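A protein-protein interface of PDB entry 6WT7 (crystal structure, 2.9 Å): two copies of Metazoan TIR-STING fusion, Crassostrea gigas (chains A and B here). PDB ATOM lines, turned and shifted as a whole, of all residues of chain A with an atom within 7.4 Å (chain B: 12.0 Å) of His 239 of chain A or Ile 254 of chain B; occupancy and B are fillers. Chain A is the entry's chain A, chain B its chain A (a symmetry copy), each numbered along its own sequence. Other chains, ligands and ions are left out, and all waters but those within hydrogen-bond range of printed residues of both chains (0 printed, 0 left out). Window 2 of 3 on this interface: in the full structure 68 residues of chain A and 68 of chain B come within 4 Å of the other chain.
Of chain B, only Ile 254 (3.5 Å) comes within 4 Å of His 239 of chain A.
Of chain A, only Ser 229, His 239, Lys 259, Thr 261 and Tyr 263 come within 4 Å of Ile 254 of chain B.
Of the printed residues of chain B, Ser 229 of chain A touches Ile 254.
No residue of chain B comes within 4 Å of Ala 231 of chain A.
Gly 241 of chain A touches none of the printed residues of chain B.
No residue of chain B comes within 4 Å of His 242 of chain A.
Lys 259 of chain A touches just these residues of chain B: Ile 253, Ile 254 and Glu 255.
Of chain B, only Gly 252, Ile 253 and Ile 254 come within 4 Å of Thr 261 of chain A.
Of the printed residues of chain A, Asp 249 of chain B touches Asp 228 (3.0 Å).
Of the printed residues of chain A, Gly 252 of chain B touches Asp 228, Thr 261 and Tyr 263.
Ala 251 of chain B touches none of the printed residues of chain A.
The nearest residue of chain A that does not touch Ile 254 of chain B is Asp 228 of chain A (4.9 Å).
No position is printed for both chains.
Of the 13 pairs that touch across the chains among the printed residues, none has its exchanged pair printed and touching as well.
Printed residues of chain B that touch a printed residue of chain A: Asp 249, Arg 250, Gly 252, Ile 253, Ile 254 and Glu 255.
Of the 19 printed residues of chain A, 6 touch a printed residue of chain B.
Hydrophobic or aromatic side chains of chain A within 4 Å of the printed part of chain B: His 239 and Tyr 263.
Asp 228 of chain A touches Arg 250 of chain B.
CD1 of Ile 254 of chain B touches OG of Ser 229 of chain A, at 3.9 Å.
His 239 of chain A touches Ile 254 of chain B (CG to CD1, 3.5 Å).
O of Lys 259 of chain A touches CG2 of Ile 253 of chain B, at 3.5 Å.
O of Glu 255 of chain B touches CE of Lys 259 of chain A (3.6 Å).
Thr 261 of chain A touches Gly 252 of chain B.
Thr 261 of chain A touches Ile 253 of chain B (OG1 to CA, 3.7 Å).
Tyr 263 of chain A touches Ile 254 of chain B (OH to CG1, 3.8 Å).
The side-chain hydroxyl of Ser 229 of chain A sits close to the backbone NH of Ala 231 of chain A.
OD1 of Asp 249 of chain B sits at hydrogen-bond distance from N of Glu 255 of chain B, at 2.8 Å.
The backbone carbonyl oxygen (O) of Asp 228 of chain A lies within hydrogen-bond range of the backbone NH (N) of Gly 252 of chain B, 3.3 Å away.
The side-chain hydroxyl (OG1) of Thr 261 of chain A is in hydrogen-bond range of the backbone NH (N) of Ile 254 of chain B (3.2 Å).
The side-chain carboxylate (OD1) of Asp 228 of chain A sits close to the backbone carbonyl oxygen (O) of Asp 249 of chain B.
NZ of Lys 259 of chain A lies close to O of Ile 254 of chain B, at 2.3 Å.
The backbone carbonyl oxygen (O) of Gly 252 of chain B sits close to the side-chain hydroxyl (OH) of Tyr 263 of chain A.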
ATOM      1  N   ASP A 228       2.516   8.893   2.751  1.00  0.00           N
ATOM      2  CA  ASP A 228       2.709   7.662   1.992  1.00  0.00           C
ATOM      3  C   ASP A 228       3.566   7.907   0.759  1.00  0.00           C
ATOM      4  O   ASP A 228       4.376   7.055   0.376  1.00  0.00           O
ATOM      5  CB  ASP A 228       1.356   7.074   1.595  1.00  0.00           C
ATOM      6  CG  ASP A 228       0.532   6.650   2.793  1.00  0.00           C
ATOM      7  OD1 ASP A 228       1.118   6.120   3.762  1.00  0.00           O
ATOM      8  OD2 ASP A 228      -0.703   6.842   2.767  1.00  0.00           O
ATOM      9  N   SER A 229       3.405   9.067   0.131  1.00  0.00           N
ATOM     10  CA  SER A 229       4.180   9.444  -1.041  1.00  0.00           C
ATOM     11  C   SER A 229       4.379  10.950  -1.017  1.00  0.00           C
ATOM     12  O   SER A 229       3.459  11.694  -0.668  1.00  0.00           O
ATOM     13  CB  SER A 229       3.482   9.016  -2.338  1.00  0.00           C
ATOM     14  OG  SER A 229       4.013   9.695  -3.464  1.00  0.00           O
ATOM     15  N   ILE A 230       5.582  11.394  -1.388  1.00  0.00           N
ATOM     16  CA  ILE A 230       5.846  12.829  -1.450  1.00  0.00           C
ATOM     17  C   ILE A 230       4.900  13.502  -2.436  1.00  0.00           C
ATOM     18  O   ILE A 230       4.590  14.692  -2.301  1.00  0.00           O
ATOM     19  CB  ILE A 230       7.323  13.088  -1.807  1.00  0.00           C
ATOM     20  CG1 ILE A 230       8.243  12.325  -0.852  1.00  0.00           C
ATOM     21  CG2 ILE A 230       7.641  14.574  -1.747  1.00  0.00           C
ATOM     22  CD1 ILE A 230       9.710  12.643  -1.035  1.00  0.00           C
ATOM     23  N   ALA A 231       4.405  12.750  -3.424  1.00  0.00           N
ATOM     24  CA  ALA A 231       3.394  13.264  -4.338  1.00  0.00           C
ATOM     25  C   ALA A 231       2.097  13.634  -3.632  1.00  0.00           C
ATOM     26  O   ALA A 231       1.245  14.290  -4.242  1.00  0.00           O
ATOM     27  CB  ALA A 231       3.114  12.236  -5.435  1.00  0.00           C
ATOM     28  N   LEU A 236       2.464  19.040  -7.856  1.00  0.00           N
ATOM     29  CA  LEU A 236       3.714  19.299  -8.557  1.00  0.00           C
ATOM     30  C   LEU A 236       4.737  18.188  -8.374  1.00  0.00           C
ATOM     31  O   LEU A 236       5.651  18.066  -9.198  1.00  0.00           O
ATOM     32  CB  LEU A 236       4.315  20.629  -8.087  1.00  0.00           C
ATOM     33  CG  LEU A 236       3.431  21.864  -8.276  1.00  0.00           C
ATOM     34  CD1 LEU A 236       4.095  23.103  -7.699  1.00  0.00           C
ATOM     35  CD2 LEU A 236       3.103  22.063  -9.748  1.00  0.00           C
ATOM     36  N   ILE A 237       4.611  17.384  -7.321  1.00  0.00           N
ATOM     37  CA  ILE A 237       5.498  16.248  -7.099  1.00  0.00           C
ATOM     38  C   ILE A 237       4.923  15.041  -7.827  1.00  0.00           C
ATOM     39  O   ILE A 237       3.744  14.709  -7.664  1.00  0.00           O
ATOM     40  CB  ILE A 237       5.663  15.957  -5.599  1.00  0.00           C
ATOM     41  CG1 ILE A 237       5.767  17.258  -4.802  1.00  0.00           C
ATOM     42  CG2 ILE A 237       6.894  15.096  -5.363  1.00  0.00           C
ATOM     43  CD1 ILE A 237       7.044  18.018  -5.039  1.00  0.00           C
ATOM     44  N   LYS A 238       5.756  14.380  -8.628  1.00  0.00           N
ATOM     45  CA  LYS A 238       5.332  13.239  -9.425  1.00  0.00           C
ATOM     46  C   LYS A 238       6.281  12.076  -9.179  1.00  0.00           C
ATOM     47  O   LYS A 238       7.502  12.259  -9.171  1.00  0.00           O
ATOM     48  CB  LYS A 238       5.304  13.591 -10.918  1.00  0.00           C
ATOM     49  CG  LYS A 238       4.519  12.618 -11.786  1.00  0.00           C
ATOM     50  CD  LYS A 238       3.022  12.851 -11.657  1.00  0.00           C
ATOM     51  CE  LYS A 238       2.245  12.063 -12.703  1.00  0.00           C
ATOM     52  NZ  LYS A 238       0.785  12.360 -12.653  1.00  0.00           N
ATOM     53  N   HIS A 239       5.719  10.889  -8.969  1.00  0.00           N
ATOM     54  CA  HIS A 239       6.524   9.677  -8.893  1.00  0.00           C
ATOM     55  C   HIS A 239       7.096   9.366 -10.270  1.00  0.00           C
ATOM     56  O   HIS A 239       6.343   9.126 -11.220  1.00  0.00           O
ATOM     57  CB  HIS A 239       5.680   8.513  -8.385  1.00  0.00           C
ATOM     58  CG  HIS A 239       6.330   7.176  -8.555  1.00  0.00           C
ATOM     59  ND1 HIS A 239       7.507   6.836  -7.923  1.00  0.00           N
ATOM     60  CD2 HIS A 239       5.970   6.096  -9.286  1.00  0.00           C
ATOM     61  CE1 HIS A 239       7.842   5.602  -8.258  1.00  0.00           C
ATOM     62  NE2 HIS A 239       6.927   5.131  -9.083  1.00  0.00           N
ATOM     63  N   ARG A 240       8.424   9.367 -10.382  1.00  0.00           N
ATOM     64  CA  ARG A 240       9.087   9.223 -11.673  1.00  0.00           C
ATOM     65  C   ARG A 240       9.974   7.988 -11.762  1.00  0.00           C
ATOM     66  O   ARG A 240      10.769   7.880 -12.702  1.00  0.00           O
ATOM     67  CB  ARG A 240       9.907  10.476 -11.984  1.00  0.00           C
ATOM     68  CG  ARG A 240       9.074  11.737 -12.093  1.00  0.00           C
ATOM     69  CD  ARG A 240       8.062  11.634 -13.220  1.00  0.00           C
ATOM     70  NE  ARG A 240       8.711  11.474 -14.516  1.00  0.00           N
ATOM     71  CZ  ARG A 240       9.098  12.486 -15.286  1.00  0.00           C
ATOM     72  NH1 ARG A 240       8.897  13.736 -14.889  1.00  0.00           N
ATOM     73  NH2 ARG A 240       9.684  12.250 -16.453  1.00  0.00           N
ATOM     74  N   GLY A 241       9.864   7.053 -10.819  1.00  0.00           N
ATOM     75  CA  GLY A 241      10.627   5.828 -10.877  1.00  0.00           C
ATOM     76  C   GLY A 241      11.303   5.546  -9.555  1.00  0.00           C
ATOM     77  O   GLY A 241      10.910   6.070  -8.507  1.00  0.00           O
ATOM     78  N   HIS A 242      12.333   4.704  -9.610  1.00  0.00           N
ATOM     79  CA  HIS A 242      13.048   4.293  -8.411  1.00  0.00           C
ATOM     80  C   HIS A 242      14.473   3.904  -8.776  1.00  0.00           C
ATOM     81  O   HIS A 242      14.798   3.676  -9.944  1.00  0.00           O
ATOM     82  CB  HIS A 242      12.338   3.126  -7.711  1.00  0.00           C
ATOM     83  CG  HIS A 242      12.134   1.929  -8.587  1.00  0.00           C
ATOM     84  ND1 HIS A 242      13.140   1.028  -8.864  1.00  0.00           N
ATOM     85  CD2 HIS A 242      11.040   1.489  -9.252  1.00  0.00           C
ATOM     86  CE1 HIS A 242      12.673   0.082  -9.660  1.00  0.00           C
ATOM     87  NE2 HIS A 242      11.401   0.338  -9.910  1.00  0.00           N
ATOM     88  N   LYS A 259      14.300  -0.333  -1.509  1.00  0.00           N
ATOM     89  CA  LYS A 259      14.096   0.447  -2.720  1.00  0.00           C
ATOM     90  C   LYS A 259      14.053   1.933  -2.388  1.00  0.00           C
ATOM     91  O   LYS A 259      13.484   2.336  -1.370  1.00  0.00           O
ATOM     92  CB  LYS A 259      12.803   0.027  -3.427  1.00  0.00           C
ATOM     93  CG  LYS A 259      12.639   0.598  -4.827  1.00  0.00           C
ATOM     94  CD  LYS A 259      11.545  -0.128  -5.595  1.00  0.00           C
ATOM     95  CE  LYS A 259      10.203  -0.022  -4.891  1.00  0.00           C
ATOM     96  NZ  LYS A 259       9.747   1.392  -4.787  1.00  0.00           N
ATOM     97  N   ASN A 260      14.665   2.739  -3.252  1.00  0.00           N
ATOM     98  CA  ASN A 260      14.680   4.188  -3.117  1.00  0.00           C
ATOM     99  C   ASN A 260      13.921   4.796  -4.286  1.00  0.00           C
ATOM    100  O   ASN A 260      14.223   4.500  -5.446  1.00  0.00           O
ATOM    101  CB  ASN A 260      16.114   4.720  -3.070  1.00  0.00           C
ATOM    102  CG  ASN A 260      16.926   4.108  -1.946  1.00  0.00           C
ATOM    103  OD1 ASN A 260      17.010   4.663  -0.850  1.00  0.00           O
ATOM    104  ND2 ASN A 260      17.527   2.952  -2.210  1.00  0.00           N
ATOM    105  N   THR A 261      12.946   5.646  -3.978  1.00  0.00           N
ATOM    106  CA  THR A 261      12.034   6.181  -4.981  1.00  0.00           C
ATOM    107  C   THR A 261      12.529   7.523  -5.511  1.00  0.00           C
ATOM    108  O   THR A 261      13.050   8.351  -4.759  1.00  0.00           O
ATOM    109  CB  THR A 261      10.629   6.334  -4.390  1.00  0.00           C
ATOM    110  OG1 THR A 261      10.154   5.055  -3.949  1.00  0.00           O
ATOM    111  CG2 THR A 261       9.660   6.891  -5.420  1.00  0.00           C
ATOM    112  N   ILE A 262      12.363   7.728  -6.819  1.00  0.00           N
ATOM    113  CA  ILE A 262      12.721   8.977  -7.482  1.00  0.00           C
ATOM    114  C   ILE A 262      11.452   9.782  -7.717  1.00  0.00           C
ATOM    115  O   ILE A 262      10.454   9.249  -8.222  1.00  0.00           O
ATOM    116  CB  ILE A 262      13.450   8.714  -8.812  1.00  0.00           C
ATOM    117  CG1 ILE A 262      14.632   7.765  -8.603  1.00  0.00           C
ATOM    118  CG2 ILE A 262      13.918  10.023  -9.428  1.00  0.00           C
ATOM    119  CD1 ILE A 262      15.734   8.342  -7.752  1.00  0.00           C
ATOM    120  N   TYR A 263      11.484  11.059  -7.353  1.00  0.00           N
ATOM    121  CA  TYR A 263      10.390  11.990  -7.600  1.00  0.00           C
ATOM    122  C   TYR A 263      10.877  13.125  -8.496  1.00  0.00           C
ATOM    123  O   TYR A 263      12.043  13.180  -8.894  1.00  0.00           O
ATOM    124  CB  TYR A 263       9.830  12.554  -6.291  1.00  0.00           C
ATOM    125  CG  TYR A 263       9.214  11.533  -5.365  1.00  0.00           C
ATOM    126  CD1 TYR A 263       7.884  11.162  -5.495  1.00  0.00           C
ATOM    127  CD2 TYR A 263       9.959  10.953  -4.346  1.00  0.00           C
ATOM    128  CE1 TYR A 263       7.314  10.233  -4.645  1.00  0.00           C
ATOM    129  CE2 TYR A 263       9.400  10.023  -3.491  1.00  0.00           C
ATOM    130  CZ  TYR A 263       8.076   9.668  -3.644  1.00  0.00           C
ATOM    131  OH  TYR A 263       7.512   8.743  -2.796  1.00  0.00           O
ATOM    132  N   SER A 264       9.964  14.043  -8.805  1.00  0.00           N
ATOM    133  CA  SER A 264      10.300  15.235  -9.568  1.00  0.00           C
ATOM    134  C   SER A 264       9.414  16.383  -9.110  1.00  0.00           C
ATOM    135  O   SER A 264       8.219  16.193  -8.869  1.00  0.00           O
ATOM    136  CB  SER A 264      10.131  15.010 -11.074  1.00  0.00           C
ATOM    137  OG  SER A 264       8.768  14.827 -11.409  1.00  0.00           O
ATOM    138  N   PHE A 274      14.642  16.888 -10.711  1.00  0.00           N
ATOM    139  CA  PHE A 274      14.568  15.535 -10.179  1.00  0.00           C
ATOM    140  C   PHE A 274      15.359  15.425  -8.880  1.00  0.00           C
ATOM    141  O   PHE A 274      16.221  16.253  -8.576  1.00  0.00           O
ATOM    142  CB  PHE A 274      15.097  14.523 -11.199  1.00  0.00           C
ATOM    143  CG  PHE A 274      14.121  14.191 -12.293  1.00  0.00           C
ATOM    144  CD1 PHE A 274      13.705  15.159 -13.192  1.00  0.00           C
ATOM    145  CD2 PHE A 274      13.630  12.903 -12.430  1.00  0.00           C
ATOM    146  CE1 PHE A 274      12.809  14.853 -14.200  1.00  0.00           C
ATOM    147  CE2 PHE A 274      12.735  12.589 -13.437  1.00  0.00           C
ATOM    148  CZ  PHE A 274      12.325  13.566 -14.323  1.00  0.00           C
ATOM    149  N   GLY A 277      14.207  11.183  -3.012  1.00  0.00           N
ATOM    150  CA  GLY A 277      13.702  11.686  -1.752  1.00  0.00           C
ATOM    151  C   GLY A 277      12.858  10.655  -1.031  1.00  0.00           C
ATOM    152  O   GLY A 277      12.304   9.731  -1.632  1.00  0.00           O
ATOM    153  N   ILE B 245       3.207 -11.173  -0.749  1.00  0.00           N
ATOM    154  CA  ILE B 245       3.909  -9.927  -0.467  1.00  0.00           C
ATOM    155  C   ILE B 245       2.907  -8.835  -0.118  1.00  0.00           C
ATOM    156  O   ILE B 245       1.860  -8.693  -0.766  1.00  0.00           O
ATOM    157  CB  ILE B 245       4.781  -9.518  -1.668  1.00  0.00           C
ATOM    158  CG1 ILE B 245       5.808 -10.605  -1.996  1.00  0.00           C
ATOM    159  CG2 ILE B 245       5.483  -8.195  -1.401  1.00  0.00           C
ATOM    160  CD1 ILE B 245       5.371 -11.571  -3.086  1.00  0.00           C
ATOM    161  N   ILE B 246       3.223  -8.059   0.914  1.00  0.00           N
ATOM    162  CA  ILE B 246       2.417  -6.915   1.321  1.00  0.00           C
ATOM    163  C   ILE B 246       3.086  -5.664   0.765  1.00  0.00           C
ATOM    164  O   ILE B 246       4.173  -5.280   1.208  1.00  0.00           O
ATOM    165  CB  ILE B 246       2.265  -6.840   2.845  1.00  0.00           C
ATOM    166  CG1 ILE B 246       1.522  -8.072   3.367  1.00  0.00           C
ATOM    167  CG2 ILE B 246       1.541  -5.564   3.246  1.00  0.00           C
ATOM    168  CD1 ILE B 246       1.321  -8.074   4.866  1.00  0.00           C
ATOM    169  N   THR B 247       2.441  -5.034  -0.212  1.00  0.00           N
ATOM    170  CA  THR B 247       2.976  -3.853  -0.874  1.00  0.00           C
ATOM    171  C   THR B 247       2.266  -2.611  -0.356  1.00  0.00           C
ATOM    172  O   THR B 247       1.033  -2.536  -0.385  1.00  0.00           O
ATOM    173  CB  THR B 247       2.818  -3.966  -2.390  1.00  0.00           C
ATOM    174  OG1 THR B 247       3.699  -4.981  -2.886  1.00  0.00           O
ATOM    175  CG2 THR B 247       3.142  -2.645  -3.065  1.00  0.00           C
ATOM    176  N   LYS B 248       3.046  -1.639   0.114  1.00  0.00           N
ATOM    177  CA  LYS B 248       2.492  -0.449   0.741  1.00  0.00           C
ATOM    178  C   LYS B 248       3.412   0.736   0.484  1.00  0.00           C
ATOM    179  O   LYS B 248       4.636   0.613   0.580  1.00  0.00           O
ATOM    180  CB  LYS B 248       2.306  -0.663   2.248  1.00  0.00           C
ATOM    181  CG  LYS B 248       1.670   0.504   2.983  1.00  0.00           C
ATOM    182  CD  LYS B 248       1.459   0.168   4.452  1.00  0.00           C
ATOM    183  CE  LYS B 248       0.854   1.338   5.214  1.00  0.00           C
ATOM    184  NZ  LYS B 248       0.647   1.014   6.655  1.00  0.00           N
ATOM    185  N   ASP B 249       2.815   1.878   0.148  1.00  0.00           N
ATOM    186  CA  ASP B 249       3.555   3.131   0.039  1.00  0.00           C
ATOM    187  C   ASP B 249       3.693   3.720   1.436  1.00  0.00           C
ATOM    188  O   ASP B 249       2.714   4.207   2.008  1.00  0.00           O
ATOM    189  CB  ASP B 249       2.844   4.106  -0.896  1.00  0.00           C
ATOM    190  CG  ASP B 249       2.554   3.507  -2.257  1.00  0.00           C
ATOM    191  OD1 ASP B 249       3.165   2.473  -2.597  1.00  0.00           O
ATOM    192  OD2 ASP B 249       1.717   4.076  -2.990  1.00  0.00           O
ATOM    193  N   ARG B 250       4.898   3.670   1.993  1.00  0.00           N
ATOM    194  CA  ARG B 250       5.135   4.140   3.349  1.00  0.00           C
ATOM    195  C   ARG B 250       6.392   4.996   3.389  1.00  0.00           C
ATOM    196  O   ARG B 250       7.390   4.679   2.733  1.00  0.00           O
ATOM    197  CB  ARG B 250       5.264   2.964   4.330  1.00  0.00           C
ATOM    198  CG  ARG B 250       5.284   3.377   5.791  1.00  0.00           C
ATOM    199  CD  ARG B 250       5.357   2.171   6.711  1.00  0.00           C
ATOM    200  NE  ARG B 250       5.614   2.566   8.092  1.00  0.00           N
ATOM    201  CZ  ARG B 250       4.666   2.813   8.990  1.00  0.00           C
ATOM    202  NH1 ARG B 250       4.997   3.172  10.224  1.00  0.00           N
ATOM    203  NH2 ARG B 250       3.387   2.698   8.656  1.00  0.00           N
ATOM    204  N   ALA B 251       6.326   6.088   4.156  1.00  0.00           N
ATOM    205  CA  ALA B 251       7.461   6.986   4.379  1.00  0.00           C
ATOM    206  C   ALA B 251       8.002   7.565   3.076  1.00  0.00           C
ATOM    207  O   ALA B 251       9.189   7.886   2.973  1.00  0.00           O
ATOM    208  CB  ALA B 251       8.581   6.286   5.152  1.00  0.00           C
ATOM    209  N   GLY B 252       7.140   7.709   2.072  1.00  0.00           N
ATOM    210  CA  GLY B 252       7.572   8.216   0.788  1.00  0.00           C
ATOM    211  C   GLY B 252       8.216   7.197  -0.120  1.00  0.00           C
ATOM    212  O   GLY B 252       8.678   7.563  -1.207  1.00  0.00           O
ATOM    213  N   ILE B 253       8.269   5.933   0.285  1.00  0.00           N
ATOM    214  CA  ILE B 253       8.804   4.859  -0.542  1.00  0.00           C
ATOM    215  C   ILE B 253       7.622   4.117  -1.148  1.00  0.00           C
ATOM    216  O   ILE B 253       6.871   3.436  -0.440  1.00  0.00           O
ATOM    217  CB  ILE B 253       9.707   3.916   0.262  1.00  0.00           C
ATOM    218  CG1 ILE B 253      10.935   4.669   0.772  1.00  0.00           C
ATOM    219  CG2 ILE B 253      10.132   2.733  -0.593  1.00  0.00           C
ATOM    220  CD1 ILE B 253      11.765   5.286  -0.332  1.00  0.00           C
ATOM    221  N   ILE B 254       7.454   4.246  -2.458  1.00  0.00           N
ATOM    222  CA  ILE B 254       6.328   3.626  -3.144  1.00  0.00           C
ATOM    223  C   ILE B 254       6.627   2.151  -3.367  1.00  0.00           C
ATOM    224  O   ILE B 254       7.730   1.785  -3.792  1.00  0.00           O
ATOM    225  CB  ILE B 254       6.036   4.353  -4.464  1.00  0.00           C
ATOM    226  CG1 ILE B 254       5.528   5.767  -4.176  1.00  0.00           C
ATOM    227  CG2 ILE B 254       5.033   3.574  -5.302  1.00  0.00           C
ATOM    228  CD1 ILE B 254       5.096   6.526  -5.399  1.00  0.00           C
ATOM    229  N   GLU B 255       5.646   1.298  -3.058  1.00  0.00           N
ATOM    230  CA  GLU B 255       5.737  -0.151  -3.245  1.00  0.00           C
ATOM    231  C   GLU B 255       6.845  -0.760  -2.383  1.00  0.00           C
ATOM    232  O   GLU B 255       7.677  -1.532  -2.859  1.00  0.00           O
ATOM    233  CB  GLU B 255       5.931  -0.513  -4.721  1.00  0.00           C
ATOM    234  CG  GLU B 255       4.749  -0.154  -5.603  1.00  0.00           C
ATOM    235  CD  GLU B 255       4.987  -0.498  -7.060  1.00  0.00           C
ATOM    236  OE1 GLU B 255       6.087  -0.997  -7.379  1.00  0.00           O
ATOM    237  OE2 GLU B 255       4.075  -0.269  -7.882  1.00  0.00           O
ATOM    238  N   ARG B 256       6.843  -0.408  -1.099  1.00  0.00           N
ATOM    239  CA  ARG B 256       7.733  -1.044  -0.137  1.00  0.00           C
ATOM    240  C   ARG B 256       7.187  -2.425   0.203  1.00  0.00           C
ATOM    241  O   ARG B 256       6.030  -2.555   0.616  1.00  0.00           O
ATOM    242  CB  ARG B 256       7.869  -0.185   1.117  1.00  0.00           C
ATOM    243  CG  ARG B 256       8.733  -0.803   2.203  1.00  0.00           C
ATOM    244  CD  ARG B 256       9.002   0.194   3.320  1.00  0.00           C
ATOM    245  NE  ARG B 256       9.624  -0.433   4.481  1.00  0.00           N
ATOM    246  CZ  ARG B 256       9.909   0.208   5.610  1.00  0.00           C
ATOM    247  NH1 ARG B 256       9.627   1.499   5.728  1.00  0.00           N
ATOM    248  NH2 ARG B 256      10.473  -0.440   6.621  1.00  0.00           N
ATOM    249  N   GLN B 257       8.011  -3.452   0.018  1.00  0.00           N
ATOM    250  CA  GLN B 257       7.576  -4.833   0.182  1.00  0.00           C
ATOM    251  C   GLN B 257       7.766  -5.293   1.621  1.00  0.00           C
ATOM    252  O   GLN B 257       8.842  -5.113   2.203  1.00  0.00           O
ATOM    253  CB  GLN B 257       8.342  -5.761  -0.762  1.00  0.00           C
ATOM    254  CG  GLN B 257       7.991  -5.604  -2.230  1.00  0.00           C
ATOM    255  CD  GLN B 257       8.518  -6.751  -3.068  1.00  0.00           C
ATOM    256  OE1 GLN B 257       9.178  -7.657  -2.554  1.00  0.00           O
ATOM    257  NE2 GLN B 257       8.229  -6.721  -4.364  1.00  0.00           N
ATOM    258  N   TYR B 258       6.721  -5.893   2.185  1.00  0.00           N
ATOM    259  CA  TYR B 258       6.777  -6.560   3.483  1.00  0.00           C
ATOM    260  C   TYR B 258       6.499  -8.038   3.229  1.00  0.00           C
ATOM    261  O   TYR B 258       5.348  -8.431   3.007  1.00  0.00           O
ATOM    262  CB  TYR B 258       5.777  -5.957   4.464  1.00  0.00           C
ATOM    263  CG  TYR B 258       6.081  -4.528   4.855  1.00  0.00           C
ATOM    264  CD1 TYR B 258       5.725  -3.469   4.028  1.00  0.00           C
ATOM    265  CD2 TYR B 258       6.718  -4.236   6.054  1.00  0.00           C
ATOM    266  CE1 TYR B 258       6.000  -2.163   4.382  1.00  0.00           C
ATOM    267  CE2 TYR B 258       6.995  -2.931   6.417  1.00  0.00           C
ATOM    268  CZ  TYR B 258       6.633  -1.899   5.576  1.00  0.00           C
ATOM    269  OH  TYR B 258       6.906  -0.598   5.931  1.00  0.00           O
